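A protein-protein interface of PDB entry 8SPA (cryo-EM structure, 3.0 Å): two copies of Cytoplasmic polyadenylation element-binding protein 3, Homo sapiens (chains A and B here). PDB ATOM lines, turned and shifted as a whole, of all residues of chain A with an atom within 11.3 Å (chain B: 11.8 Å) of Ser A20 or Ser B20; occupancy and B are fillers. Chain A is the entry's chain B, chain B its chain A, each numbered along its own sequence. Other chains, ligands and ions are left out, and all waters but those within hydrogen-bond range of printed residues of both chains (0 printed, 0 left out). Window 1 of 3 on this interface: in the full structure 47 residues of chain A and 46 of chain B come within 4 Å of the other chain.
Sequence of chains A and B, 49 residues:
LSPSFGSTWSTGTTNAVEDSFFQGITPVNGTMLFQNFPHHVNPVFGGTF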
ATOM      1  N   ASN A  15       7.421 -29.550  -1.531  1.00  0.00           N
ATOM      2  CA  ASN A  15       6.565 -28.610  -2.243  1.00  0.00           C
ATOM      3  C   ASN A  15       6.005 -27.601  -1.249  1.00  0.00           C
ATOM      4  O   ASN A  15       4.813 -27.619  -0.943  1.00  0.00           O
ATOM      5  CB  ASN A  15       5.447 -29.354  -2.959  1.00  0.00           C
ATOM      6  CG  ASN A  15       5.967 -30.288  -4.022  1.00  0.00           C
ATOM      7  OD1 ASN A  15       6.885 -29.951  -4.761  1.00  0.00           O
ATOM      8  ND2 ASN A  15       5.386 -31.474  -4.102  1.00  0.00           N
ATOM      9  N   ALA A  16       6.856 -26.707  -0.761  1.00  0.00           N
ATOM     10  CA  ALA A  16       6.441 -25.681   0.192  1.00  0.00           C
ATOM     11  C   ALA A  16       5.741 -24.586  -0.599  1.00  0.00           C
ATOM     12  O   ALA A  16       6.378 -23.648  -1.080  1.00  0.00           O
ATOM     13  CB  ALA A  16       7.634 -25.140   0.970  1.00  0.00           C
ATOM     14  N   VAL A  17       4.421 -24.702  -0.723  1.00  0.00           N
ATOM     15  CA  VAL A  17       3.695 -23.884  -1.689  1.00  0.00           C
ATOM     16  C   VAL A  17       3.510 -22.464  -1.174  1.00  0.00           C
ATOM     17  O   VAL A  17       3.960 -21.499  -1.801  1.00  0.00           O
ATOM     18  CB  VAL A  17       2.346 -24.529  -2.038  1.00  0.00           C
ATOM     19  CG1 VAL A  17       1.483 -23.546  -2.800  1.00  0.00           C
ATOM     20  CG2 VAL A  17       2.572 -25.776  -2.863  1.00  0.00           C
ATOM     21  N   GLU A  18       2.837 -22.307  -0.037  1.00  0.00           N
ATOM     22  CA  GLU A  18       2.333 -20.987   0.338  1.00  0.00           C
ATOM     23  C   GLU A  18       2.450 -20.820   1.848  1.00  0.00           C
ATOM     24  O   GLU A  18       1.516 -21.153   2.579  1.00  0.00           O
ATOM     25  CB  GLU A  18       0.897 -20.830  -0.132  1.00  0.00           C
ATOM     26  CG  GLU A  18       0.290 -19.481   0.123  1.00  0.00           C
ATOM     27  CD  GLU A  18      -1.114 -19.396  -0.422  1.00  0.00           C
ATOM     28  OE1 GLU A  18      -1.598 -20.404  -0.973  1.00  0.00           O
ATOM     29  OE2 GLU A  18      -1.731 -18.321  -0.320  1.00  0.00           O
ATOM     30  N   ASP A  19       3.562 -20.256   2.305  1.00  0.00           N
ATOM     31  CA  ASP A  19       3.856 -20.261   3.731  1.00  0.00           C
ATOM     32  C   ASP A  19       4.842 -19.146   4.058  1.00  0.00           C
ATOM     33  O   ASP A  19       5.234 -18.362   3.193  1.00  0.00           O
ATOM     34  CB  ASP A  19       4.369 -21.635   4.152  1.00  0.00           C
ATOM     35  CG  ASP A  19       5.584 -22.067   3.376  1.00  0.00           C
ATOM     36  OD1 ASP A  19       6.015 -21.317   2.489  1.00  0.00           O
ATOM     37  OD2 ASP A  19       6.103 -23.169   3.637  1.00  0.00           O
ATOM     38  N   SER A  20       5.228 -19.073   5.331  1.00  0.00           N
ATOM     39  CA  SER A  20       6.100 -18.023   5.837  1.00  0.00           C
ATOM     40  C   SER A  20       7.069 -18.609   6.850  1.00  0.00           C
ATOM     41  O   SER A  20       6.657 -19.344   7.751  1.00  0.00           O
ATOM     42  CB  SER A  20       5.285 -16.903   6.484  1.00  0.00           C
ATOM     43  OG  SER A  20       6.134 -15.901   7.006  1.00  0.00           O
ATOM     44  N   PHE A  21       8.350 -18.278   6.711  1.00  0.00           N
ATOM     45  CA  PHE A  21       9.404 -18.820   7.560  1.00  0.00           C
ATOM     46  C   PHE A  21      10.087 -17.690   8.312  1.00  0.00           C
ATOM     47  O   PHE A  21      10.210 -16.578   7.792  1.00  0.00           O
ATOM     48  CB  PHE A  21      10.449 -19.586   6.746  1.00  0.00           C
ATOM     49  CG  PHE A  21       9.935 -20.839   6.099  1.00  0.00           C
ATOM     50  CD1 PHE A  21       8.657 -21.296   6.335  1.00  0.00           C
ATOM     51  CD2 PHE A  21      10.744 -21.565   5.251  1.00  0.00           C
ATOM     52  CE1 PHE A  21       8.196 -22.441   5.734  1.00  0.00           C
ATOM     53  CE2 PHE A  21      10.286 -22.715   4.650  1.00  0.00           C
ATOM     54  CZ  PHE A  21       9.012 -23.152   4.892  1.00  0.00           C
ATOM     55  N   PHE A  22      10.529 -17.977   9.532  1.00  0.00           N
ATOM     56  CA  PHE A  22      11.322 -17.053  10.332  1.00  0.00           C
ATOM     57  C   PHE A  22      12.454 -17.832  10.975  1.00  0.00           C
ATOM     58  O   PHE A  22      12.326 -19.037  11.204  1.00  0.00           O
ATOM     59  CB  PHE A  22      10.486 -16.371  11.415  1.00  0.00           C
ATOM     60  CG  PHE A  22       9.456 -15.425  10.886  1.00  0.00           C
ATOM     61  CD1 PHE A  22       8.301 -15.892  10.293  1.00  0.00           C
ATOM     62  CD2 PHE A  22       9.636 -14.063  11.001  1.00  0.00           C
ATOM     63  CE1 PHE A  22       7.354 -15.021   9.813  1.00  0.00           C
ATOM     64  CE2 PHE A  22       8.689 -13.189  10.523  1.00  0.00           C
ATOM     65  CZ  PHE A  22       7.547 -13.667   9.929  1.00  0.00           C
ATOM     66  N   GLN A  23      13.560 -17.154  11.257  1.00  0.00           N
ATOM     67  CA  GLN A  23      14.690 -17.785  11.917  1.00  0.00           C
ATOM     68  C   GLN A  23      15.535 -16.718  12.592  1.00  0.00           C
ATOM     69  O   GLN A  23      15.690 -15.618  12.061  1.00  0.00           O
ATOM     70  CB  GLN A  23      15.535 -18.583  10.924  1.00  0.00           C
ATOM     71  CG  GLN A  23      16.515 -19.524  11.576  1.00  0.00           C
ATOM     72  CD  GLN A  23      16.905 -20.668  10.672  1.00  0.00           C
ATOM     73  OE1 GLN A  23      16.421 -20.779   9.549  1.00  0.00           O
ATOM     74  NE2 GLN A  23      17.791 -21.527  11.156  1.00  0.00           N
ATOM     75  N   THR A  26      13.964 -12.793  16.866  1.00  0.00           N
ATOM     76  CA  THR A  26      12.886 -12.013  16.262  1.00  0.00           C
ATOM     77  C   THR A  26      11.950 -11.496  17.346  1.00  0.00           C
ATOM     78  O   THR A  26      10.825 -11.989  17.494  1.00  0.00           O
ATOM     79  CB  THR A  26      12.116 -12.853  15.243  1.00  0.00           C
ATOM     80  OG1 THR A  26      13.040 -13.607  14.450  1.00  0.00           O
ATOM     81  CG2 THR A  26      11.285 -11.968  14.337  1.00  0.00           C
ATOM     82  N   MET A  32       0.995  -8.971  14.719  1.00  0.00           N
ATOM     83  CA  MET A  32       1.160  -9.875  13.591  1.00  0.00           C
ATOM     84  C   MET A  32      -0.155 -10.604  13.369  1.00  0.00           C
ATOM     85  O   MET A  32      -0.724 -11.160  14.314  1.00  0.00           O
ATOM     86  CB  MET A  32       2.284 -10.876  13.841  1.00  0.00           C
ATOM     87  CG  MET A  32       3.640 -10.243  14.049  1.00  0.00           C
ATOM     88  SD  MET A  32       4.980 -11.408  13.753  1.00  0.00           S
ATOM     89  CE  MET A  32       5.012 -11.434  11.965  1.00  0.00           C
ATOM     90  N   LEU A  33      -0.633 -10.605  12.131  1.00  0.00           N
ATOM     91  CA  LEU A  33      -1.920 -11.195  11.799  1.00  0.00           C
ATOM     92  C   LEU A  33      -1.724 -12.237  10.707  1.00  0.00           C
ATOM     93  O   LEU A  33      -1.047 -11.978   9.710  1.00  0.00           O
ATOM     94  CB  LEU A  33      -2.909 -10.116  11.353  1.00  0.00           C
ATOM     95  CG  LEU A  33      -4.376 -10.482  11.125  1.00  0.00           C
ATOM     96  CD1 LEU A  33      -5.237  -9.255  11.346  1.00  0.00           C
ATOM     97  CD2 LEU A  33      -4.625 -11.044   9.741  1.00  0.00           C
ATOM     98  N   PHE A  34      -2.322 -13.408  10.901  1.00  0.00           N
ATOM     99  CA  PHE A  34      -2.285 -14.494   9.927  1.00  0.00           C
ATOM    100  C   PHE A  34      -3.708 -14.994   9.755  1.00  0.00           C
ATOM    101  O   PHE A  34      -4.287 -15.549  10.693  1.00  0.00           O
ATOM    102  CB  PHE A  34      -1.384 -15.636  10.391  1.00  0.00           C
ATOM    103  CG  PHE A  34       0.017 -15.221  10.703  1.00  0.00           C
ATOM    104  CD1 PHE A  34       0.337 -14.711  11.945  1.00  0.00           C
ATOM    105  CD2 PHE A  34       1.020 -15.372   9.769  1.00  0.00           C
ATOM    106  CE1 PHE A  34       1.626 -14.340  12.240  1.00  0.00           C
ATOM    107  CE2 PHE A  34       2.311 -15.002  10.061  1.00  0.00           C
ATOM    108  CZ  PHE A  34       2.615 -14.485  11.298  1.00  0.00           C
ATOM    109  N   GLN A  35      -4.278 -14.807   8.570  1.00  0.00           N
ATOM    110  CA  GLN A  35      -5.630 -15.272   8.297  1.00  0.00           C
ATOM    111  C   GLN A  35      -5.667 -15.931   6.931  1.00  0.00           C
ATOM    112  O   GLN A  35      -5.038 -15.448   5.987  1.00  0.00           O
ATOM    113  CB  GLN A  35      -6.634 -14.124   8.404  1.00  0.00           C
ATOM    114  CG  GLN A  35      -6.475 -13.029   7.390  1.00  0.00           C
ATOM    115  CD  GLN A  35      -7.468 -11.913   7.616  1.00  0.00           C
ATOM    116  OE1 GLN A  35      -8.309 -11.991   8.507  1.00  0.00           O
ATOM    117  NE2 GLN A  35      -7.370 -10.862   6.815  1.00  0.00           N
ATOM    118  N   ASN A  36      -6.388 -17.044   6.836  1.00  0.00           N
ATOM    119  CA  ASN A  36      -6.381 -17.896   5.657  1.00  0.00           C
ATOM    120  C   ASN A  36      -7.800 -18.346   5.362  1.00  0.00           C
ATOM    121  O   ASN A  36      -8.465 -18.907   6.237  1.00  0.00           O
ATOM    122  CB  ASN A  36      -5.485 -19.110   5.883  1.00  0.00           C
ATOM    123  CG  ASN A  36      -4.025 -18.745   5.942  1.00  0.00           C
ATOM    124  OD1 ASN A  36      -3.550 -17.929   5.159  1.00  0.00           O
ATOM    125  ND2 ASN A  36      -3.301 -19.349   6.873  1.00  0.00           N
ATOM    126  N   ASN B  15       4.601 -32.016   1.794  1.00  0.00           N
ATOM    127  CA  ASN B  15       3.761 -31.029   1.127  1.00  0.00           C
ATOM    128  C   ASN B  15       3.271 -30.021   2.158  1.00  0.00           C
ATOM    129  O   ASN B  15       2.088 -30.000   2.499  1.00  0.00           O
ATOM    130  CB  ASN B  15       2.595 -31.717   0.431  1.00  0.00           C
ATOM    131  CG  ASN B  15       3.046 -32.648  -0.665  1.00  0.00           C
ATOM    132  OD1 ASN B  15       3.954 -32.330  -1.425  1.00  0.00           O
ATOM    133  ND2 ASN B  15       2.419 -33.810  -0.749  1.00  0.00           N
ATOM    134  N   ALA B  16       4.169 -29.169   2.636  1.00  0.00           N
ATOM    135  CA  ALA B  16       3.823 -28.148   3.620  1.00  0.00           C
ATOM    136  C   ALA B  16       3.141 -27.012   2.872  1.00  0.00           C
ATOM    137  O   ALA B  16       3.799 -26.089   2.389  1.00  0.00           O
ATOM    138  CB  ALA B  16       5.058 -27.668   4.372  1.00  0.00           C
ATOM    139  N   VAL B  17       1.814 -27.075   2.786  1.00  0.00           N
ATOM    140  CA  VAL B  17       1.091 -26.212   1.858  1.00  0.00           C
ATOM    141  C   VAL B  17       0.977 -24.797   2.405  1.00  0.00           C
ATOM    142  O   VAL B  17       1.444 -23.837   1.784  1.00  0.00           O
ATOM    143  CB  VAL B  17      -0.291 -26.799   1.539  1.00  0.00           C
ATOM    144  CG1 VAL B  17      -1.138 -25.769   0.823  1.00  0.00           C
ATOM    145  CG2 VAL B  17      -0.137 -28.036   0.684  1.00  0.00           C
ATOM    146  N   GLU B  18       0.344 -24.637   3.566  1.00  0.00           N
ATOM    147  CA  GLU B  18      -0.097 -23.307   3.981  1.00  0.00           C
ATOM    148  C   GLU B  18       0.070 -23.175   5.490  1.00  0.00           C
ATOM    149  O   GLU B  18      -0.853 -23.487   6.243  1.00  0.00           O
ATOM    150  CB  GLU B  18      -1.539 -23.087   3.558  1.00  0.00           C
ATOM    151  CG  GLU B  18      -2.087 -21.722   3.858  1.00  0.00           C
ATOM    152  CD  GLU B  18      -3.503 -21.573   3.358  1.00  0.00           C
ATOM    153  OE1 GLU B  18      -4.041 -22.551   2.803  1.00  0.00           O
ATOM    154  OE2 GLU B  18      -4.075 -20.477   3.500  1.00  0.00           O
ATOM    155  N   ASP B  19       1.216 -22.663   5.923  1.00  0.00           N
ATOM    156  CA  ASP B  19       1.553 -22.707   7.339  1.00  0.00           C
ATOM    157  C   ASP B  19       2.590 -21.637   7.657  1.00  0.00           C
ATOM    158  O   ASP B  19       2.986 -20.850   6.794  1.00  0.00           O
ATOM    159  CB  ASP B  19       2.026 -24.108   7.719  1.00  0.00           C
ATOM    160  CG  ASP B  19       3.200 -24.569   6.897  1.00  0.00           C
ATOM    161  OD1 ASP B  19       3.632 -23.819   6.011  1.00  0.00           O
ATOM    162  OD2 ASP B  19       3.684 -25.695   7.121  1.00  0.00           O
ATOM    163  N   SER B  20       3.016 -21.605   8.917  1.00  0.00           N
ATOM    164  CA  SER B  20       3.943 -20.598   9.418  1.00  0.00           C
ATOM    165  C   SER B  20       4.919 -21.240  10.389  1.00  0.00           C
ATOM    166  O   SER B  20       4.505 -21.978  11.287  1.00  0.00           O
ATOM    167  CB  SER B  20       3.191 -19.463  10.110  1.00  0.00           C
ATOM    168  OG  SER B  20       4.094 -18.503  10.625  1.00  0.00           O
ATOM    169  N   PHE B  21       6.207 -20.955  10.217  1.00  0.00           N
ATOM    170  CA  PHE B  21       7.263 -21.554  11.023  1.00  0.00           C
ATOM    171  C   PHE B  21       8.013 -20.465  11.775  1.00  0.00           C
ATOM    172  O   PHE B  21       8.161 -19.349  11.271  1.00  0.00           O
ATOM    173  CB  PHE B  21       8.254 -22.342  10.161  1.00  0.00           C
ATOM    174  CG  PHE B  21       7.674 -23.562   9.507  1.00  0.00           C
ATOM    175  CD1 PHE B  21       6.387 -23.974   9.774  1.00  0.00           C
ATOM    176  CD2 PHE B  21       8.429 -24.301   8.622  1.00  0.00           C
ATOM    177  CE1 PHE B  21       5.865 -25.088   9.166  1.00  0.00           C
ATOM    178  CE2 PHE B  21       7.909 -25.419   8.013  1.00  0.00           C
ATOM    179  CZ  PHE B  21       6.627 -25.812   8.286  1.00  0.00           C
ATOM    180  N   PHE B  22       8.479 -20.793  12.976  1.00  0.00           N
ATOM    181  CA  PHE B  22       9.330 -19.916  13.768  1.00  0.00           C
ATOM    182  C   PHE B  22      10.450 -20.750  14.361  1.00  0.00           C
ATOM    183  O   PHE B  22      10.284 -21.953  14.572  1.00  0.00           O
ATOM    184  CB  PHE B  22       8.554 -19.225  14.888  1.00  0.00           C
ATOM    185  CG  PHE B  22       7.546 -18.230  14.410  1.00  0.00           C
ATOM    186  CD1 PHE B  22       6.357 -18.642  13.843  1.00  0.00           C
ATOM    187  CD2 PHE B  22       7.780 -16.879  14.544  1.00  0.00           C
ATOM    188  CE1 PHE B  22       5.429 -17.726  13.409  1.00  0.00           C
ATOM    189  CE2 PHE B  22       6.854 -15.959  14.113  1.00  0.00           C
ATOM    190  CZ  PHE B  22       5.677 -16.383  13.545  1.00  0.00           C
ATOM    191  N   GLN B  23      11.590 -20.119  14.621  1.00  0.00           N
ATOM    192  CA  GLN B  23      12.714 -20.806  15.235  1.00  0.00           C
ATOM    193  C   GLN B  23      13.618 -19.785  15.903  1.00  0.00           C
ATOM    194  O   GLN B  23      13.800 -18.680  15.389  1.00  0.00           O
ATOM    195  CB  GLN B  23      13.497 -21.614  14.201  1.00  0.00           C
ATOM    196  CG  GLN B  23      14.459 -22.605  14.804  1.00  0.00           C
ATOM    197  CD  GLN B  23      14.779 -23.745  13.868  1.00  0.00           C
ATOM    198  OE1 GLN B  23      14.257 -23.814  12.758  1.00  0.00           O
ATOM    199  NE2 GLN B  23      15.646 -24.646  14.307  1.00  0.00           N
ATOM    200  N   GLY B  24      14.180 -20.155  17.045  1.00  0.00           N
ATOM    201  CA  GLY B  24      15.071 -19.275  17.775  1.00  0.00           C
ATOM    202  C   GLY B  24      14.333 -18.417  18.781  1.00  0.00           C
ATOM    203  O   GLY B  24      13.106 -18.463  18.918  1.00  0.00           O
ATOM    204  N   THR B  26      12.328 -15.890  20.297  1.00  0.00           N
ATOM    205  CA  THR B  26      11.262 -15.059  19.741  1.00  0.00           C
ATOM    206  C   THR B  26      10.379 -14.529  20.864  1.00  0.00           C
ATOM    207  O   THR B  26       9.242 -14.982  21.037  1.00  0.00           O
ATOM    208  CB  THR B  26      10.430 -15.849  18.731  1.00  0.00           C
ATOM    209  OG1 THR B  26      11.302 -16.621  17.896  1.00  0.00           O
ATOM    210  CG2 THR B  26       9.607 -14.914  17.867  1.00  0.00           C
ATOM    211  N   MET B  32      -0.545 -11.542  18.622  1.00  0.00           N
ATOM    212  CA  MET B  32      -0.449 -12.428  17.473  1.00  0.00           C
ATOM    213  C   MET B  32      -1.796 -13.103  17.278  1.00  0.00           C
ATOM    214  O   MET B  32      -2.358 -13.656  18.229  1.00  0.00           O
ATOM    215  CB  MET B  32       0.644 -13.476  17.670  1.00  0.00           C
ATOM    216  CG  MET B  32       2.029 -12.898  17.847  1.00  0.00           C
ATOM    217  SD  MET B  32       3.314 -14.106  17.488  1.00  0.00           S
ATOM    218  CE  MET B  32       3.292 -14.098  15.699  1.00  0.00           C
ATOM    219  N   LEU B  33      -2.311 -13.061  16.055  1.00  0.00           N
ATOM    220  CA  LEU B  33      -3.628 -13.596  15.751  1.00  0.00           C
ATOM    221  C   LEU B  33      -3.506 -14.621  14.635  1.00  0.00           C
ATOM    222  O   LEU B  33      -2.849 -14.367  13.622  1.00  0.00           O
ATOM    223  CB  LEU B  33      -4.588 -12.470  15.356  1.00  0.00           C
ATOM    224  CG  LEU B  33      -6.075 -12.777  15.167  1.00  0.00           C
ATOM    225  CD1 LEU B  33      -6.880 -11.523  15.437  1.00  0.00           C
ATOM    226  CD2 LEU B  33      -6.387 -13.302  13.781  1.00  0.00           C
ATOM    227  N   PHE B  34      -4.142 -15.774  14.824  1.00  0.00           N
ATOM    228  CA  PHE B  34      -4.176 -16.840  13.829  1.00  0.00           C
ATOM    229  C   PHE B  34      -5.621 -17.282  13.691  1.00  0.00           C
ATOM    230  O   PHE B  34      -6.192 -17.833  14.636  1.00  0.00           O
ATOM    231  CB  PHE B  34      -3.305 -18.024  14.243  1.00  0.00           C
ATOM    232  CG  PHE B  34      -1.881 -17.669  14.520  1.00  0.00           C
ATOM    233  CD1 PHE B  34      -1.503 -17.196  15.760  1.00  0.00           C
ATOM    234  CD2 PHE B  34      -0.913 -17.838  13.553  1.00  0.00           C
ATOM    235  CE1 PHE B  34      -0.193 -16.879  16.024  1.00  0.00           C
ATOM    236  CE2 PHE B  34       0.401 -17.523  13.812  1.00  0.00           C
ATOM    237  CZ  PHE B  34       0.761 -17.043  15.049  1.00  0.00           C
ATOM    238  N   GLN B  35      -6.218 -17.050  12.528  1.00  0.00           N
ATOM    239  CA  GLN B  35      -7.595 -17.458  12.289  1.00  0.00           C
ATOM    240  C   GLN B  35      -7.698 -18.088  10.911  1.00  0.00           C
ATOM    241  O   GLN B  35      -7.080 -17.610   9.957  1.00  0.00           O
ATOM    242  CB  GLN B  35      -8.550 -16.275  12.447  1.00  0.00           C
ATOM    243  CG  GLN B  35      -8.381 -15.168  11.450  1.00  0.00           C
ATOM    244  CD  GLN B  35      -9.323 -14.020  11.727  1.00  0.00           C
ATOM    245  OE1 GLN B  35     -10.139 -14.083  12.642  1.00  0.00           O
ATOM    246  NE2 GLN B  35      -9.208 -12.957  10.944  1.00  0.00           N
ATOM    247  N   ASN B  36      -8.463 -19.172  10.817  1.00  0.00           N
ATOM    248  CA  ASN B  36      -8.523 -19.998   9.623  1.00  0.00           C
ATOM    249  C   ASN B  36      -9.967 -20.389   9.363  1.00  0.00           C
ATOM    250  O   ASN B  36     -10.627 -20.941  10.247  1.00  0.00           O
ATOM    251  CB  ASN B  36      -7.668 -21.250   9.798  1.00  0.00           C
ATOM    252  CG  ASN B  36      -6.194 -20.941   9.820  1.00  0.00           C
ATOM    253  OD1 ASN B  36      -5.712 -20.128   9.038  1.00  0.00           O
ATOM    254  ND2 ASN B  36      -5.466 -21.590  10.715  1.00  0.00           N
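Among the printed residues, merely in contact across the chains: Glu A18 with Glu B18 (3.0 Å), Thr A26 with Thr B26 (3.2 Å), Phe A34 with Phe B34 (3.4 Å), Met A32 with Met B32 (3.4 Å), Ser A20 with Ser B20 (3.4 Å), Phe A21 with Phe B21 (3.4 Å), Ala A16 with Ala B16 (3.5 Å), Phe A22 with Gln B23 (3.7 Å), Glu A18 with Asp B19 (3.7 Å), Gln A23 with Gln B23 (3.7 Å), Leu A33 with Leu B33 (3.8 Å), Asn A15 with Ala B16 (3.8 Å), Phe A34 with Met B32 (3.8 Å), Val A17 with Val B17 (3.9 Å), Asp A19 with Ala B16 (3.9 Å) and Phe A34 with Ser B20 (3.97 Å).
Ser B20 touches just these residues of chain A: Ser A20 (3.4 Å) and Phe A34 (3.97 Å).
Asp A19 touches just these residues of chain B: Ala B16 and Asp B19.
Of chain B, only Phe B21 comes within 4 Å of Phe A21.
Asp B19 touches three residues of chain A.
Of chain A, only Ser A20, Phe A21 and Phe A22 come within 4 Å of Phe B21.
Of the printed residues of chain B, Gln A23 touches Gln B23.
Printed residues of chain A within 4 Å of Glu B18: Glu A18 and Asn A36.
Of the printed residues of chain B, Val A17 touches Ala B16 (3.5 Å) and Val B17 (3.9 Å).
Of the printed residues of chain B, Glu A18 touches Val B17 (2.8 Å), Glu B18 (3.0 Å) and Asp B19 (3.7 Å).
Of the printed residues of chain B, Met A32 touches Met B32 (3.4 Å) and Leu B33 (3.0 Å).
Gly B24 touches none of the printed residues of chain A.
The nearest residue of chain B that does not touch Ser A20 is Phe B22 (5.7 Å).
The backbone carbonyl oxygen (O) of Gly B24 is in hydrogen-bond range of the side-chain hydroxyl (OG1) of Thr B26, 2.8 Å away.
Printed residues of chain A that touch a printed residue of chain B: Asn A15, Ala A16, Val A17, Glu A18, Asp A19, Ser A20, Phe A21, Phe A22, Gln A23, Thr A26, Met A32, Leu A33, Phe A34, Gln A35 and Asn A36.
Hydrophobic or aromatic side chains of chain A within 4 Å of the printed part of chain B: Val A17, Phe A21, Phe A22, Met A32 and Phe A34.
Printed residues of chain B that touch a printed residue of chain A: Asn B15, Ala B16, Val B17, Glu B18, Asp B19, Ser B20, Phe B21, Gln B23, Thr B26, Met B32, Leu B33, Phe B34, Gln B35 and Asn B36.
Ser B20 touches its own counterpart, Ser A20.
Phe A22 touches Gln B23, but with the chains exchanged Gln A23 does not touch Phe B22 (5.6 Å).
Met A32 touches Leu B33, but with the chains exchanged Leu A33 does not touch Met B32 (5.6 Å).
Asn A36 touches its own counterpart, Asn B36.
Of the 30 pairs that touch across the chains among the printed residues, 14 have their exchanged pair printed and touching as well.
The backbone NH (N) of Phe A34 is in hydrogen-bond range of the backbone carbonyl oxygen (O) of Leu B33 (2.9 Å).
The backbone carbonyl oxygen (O) of Ser A20 is in hydrogen-bond range of the backbone NH (N) of Phe B21 (3.0 Å).
The backbone carbonyl oxygen of Phe B21 is in hydrogen-bond range of the backbone NH of Phe A22, 3.2 Å away.
O of Met A32 is in hydrogen-bond range of N of Leu B33 (3.0 Å).
OD1 of Asn B15 lies within hydrogen-bond range of ND2 of Asn A15 (3.2 Å).
The backbone NH of Val A17 is in hydrogen-bond range of the backbone carbonyl oxygen of Ala B16 (3.5 Å).
The backbone NH (N) of Gln B35 sits at hydrogen-bond distance from the backbone carbonyl oxygen (O) of Phe A34.
OD1 of Asn B36 lies close to ND2 of Asn A36 (3.3 Å).
The backbone carbonyl oxygen (O) of Asp B19 lies within hydrogen-bond range of the backbone NH (N) of Ser A20 (3.2 Å).
The side-chain amide nitrogen (NE2) of Gln B35 lies within hydrogen-bond range of the side-chain amide oxygen (OE1) of Gln A35, 2.8 Å away.
The backbone NH (N) of Glu A18 is in hydrogen-bond range of the backbone carbonyl oxygen (O) of Val B17 (2.8 Å).
OE2 of Glu B18 sits close to OD1 of Asn A36 (3.1 Å).
O of Gln B35 lies within hydrogen-bond range of N of Asn A36 (3.2 Å).
The side-chain carboxylate of Asp A19 lies close to the side-chain carboxylate of Asp B19, at 3.5 Å.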
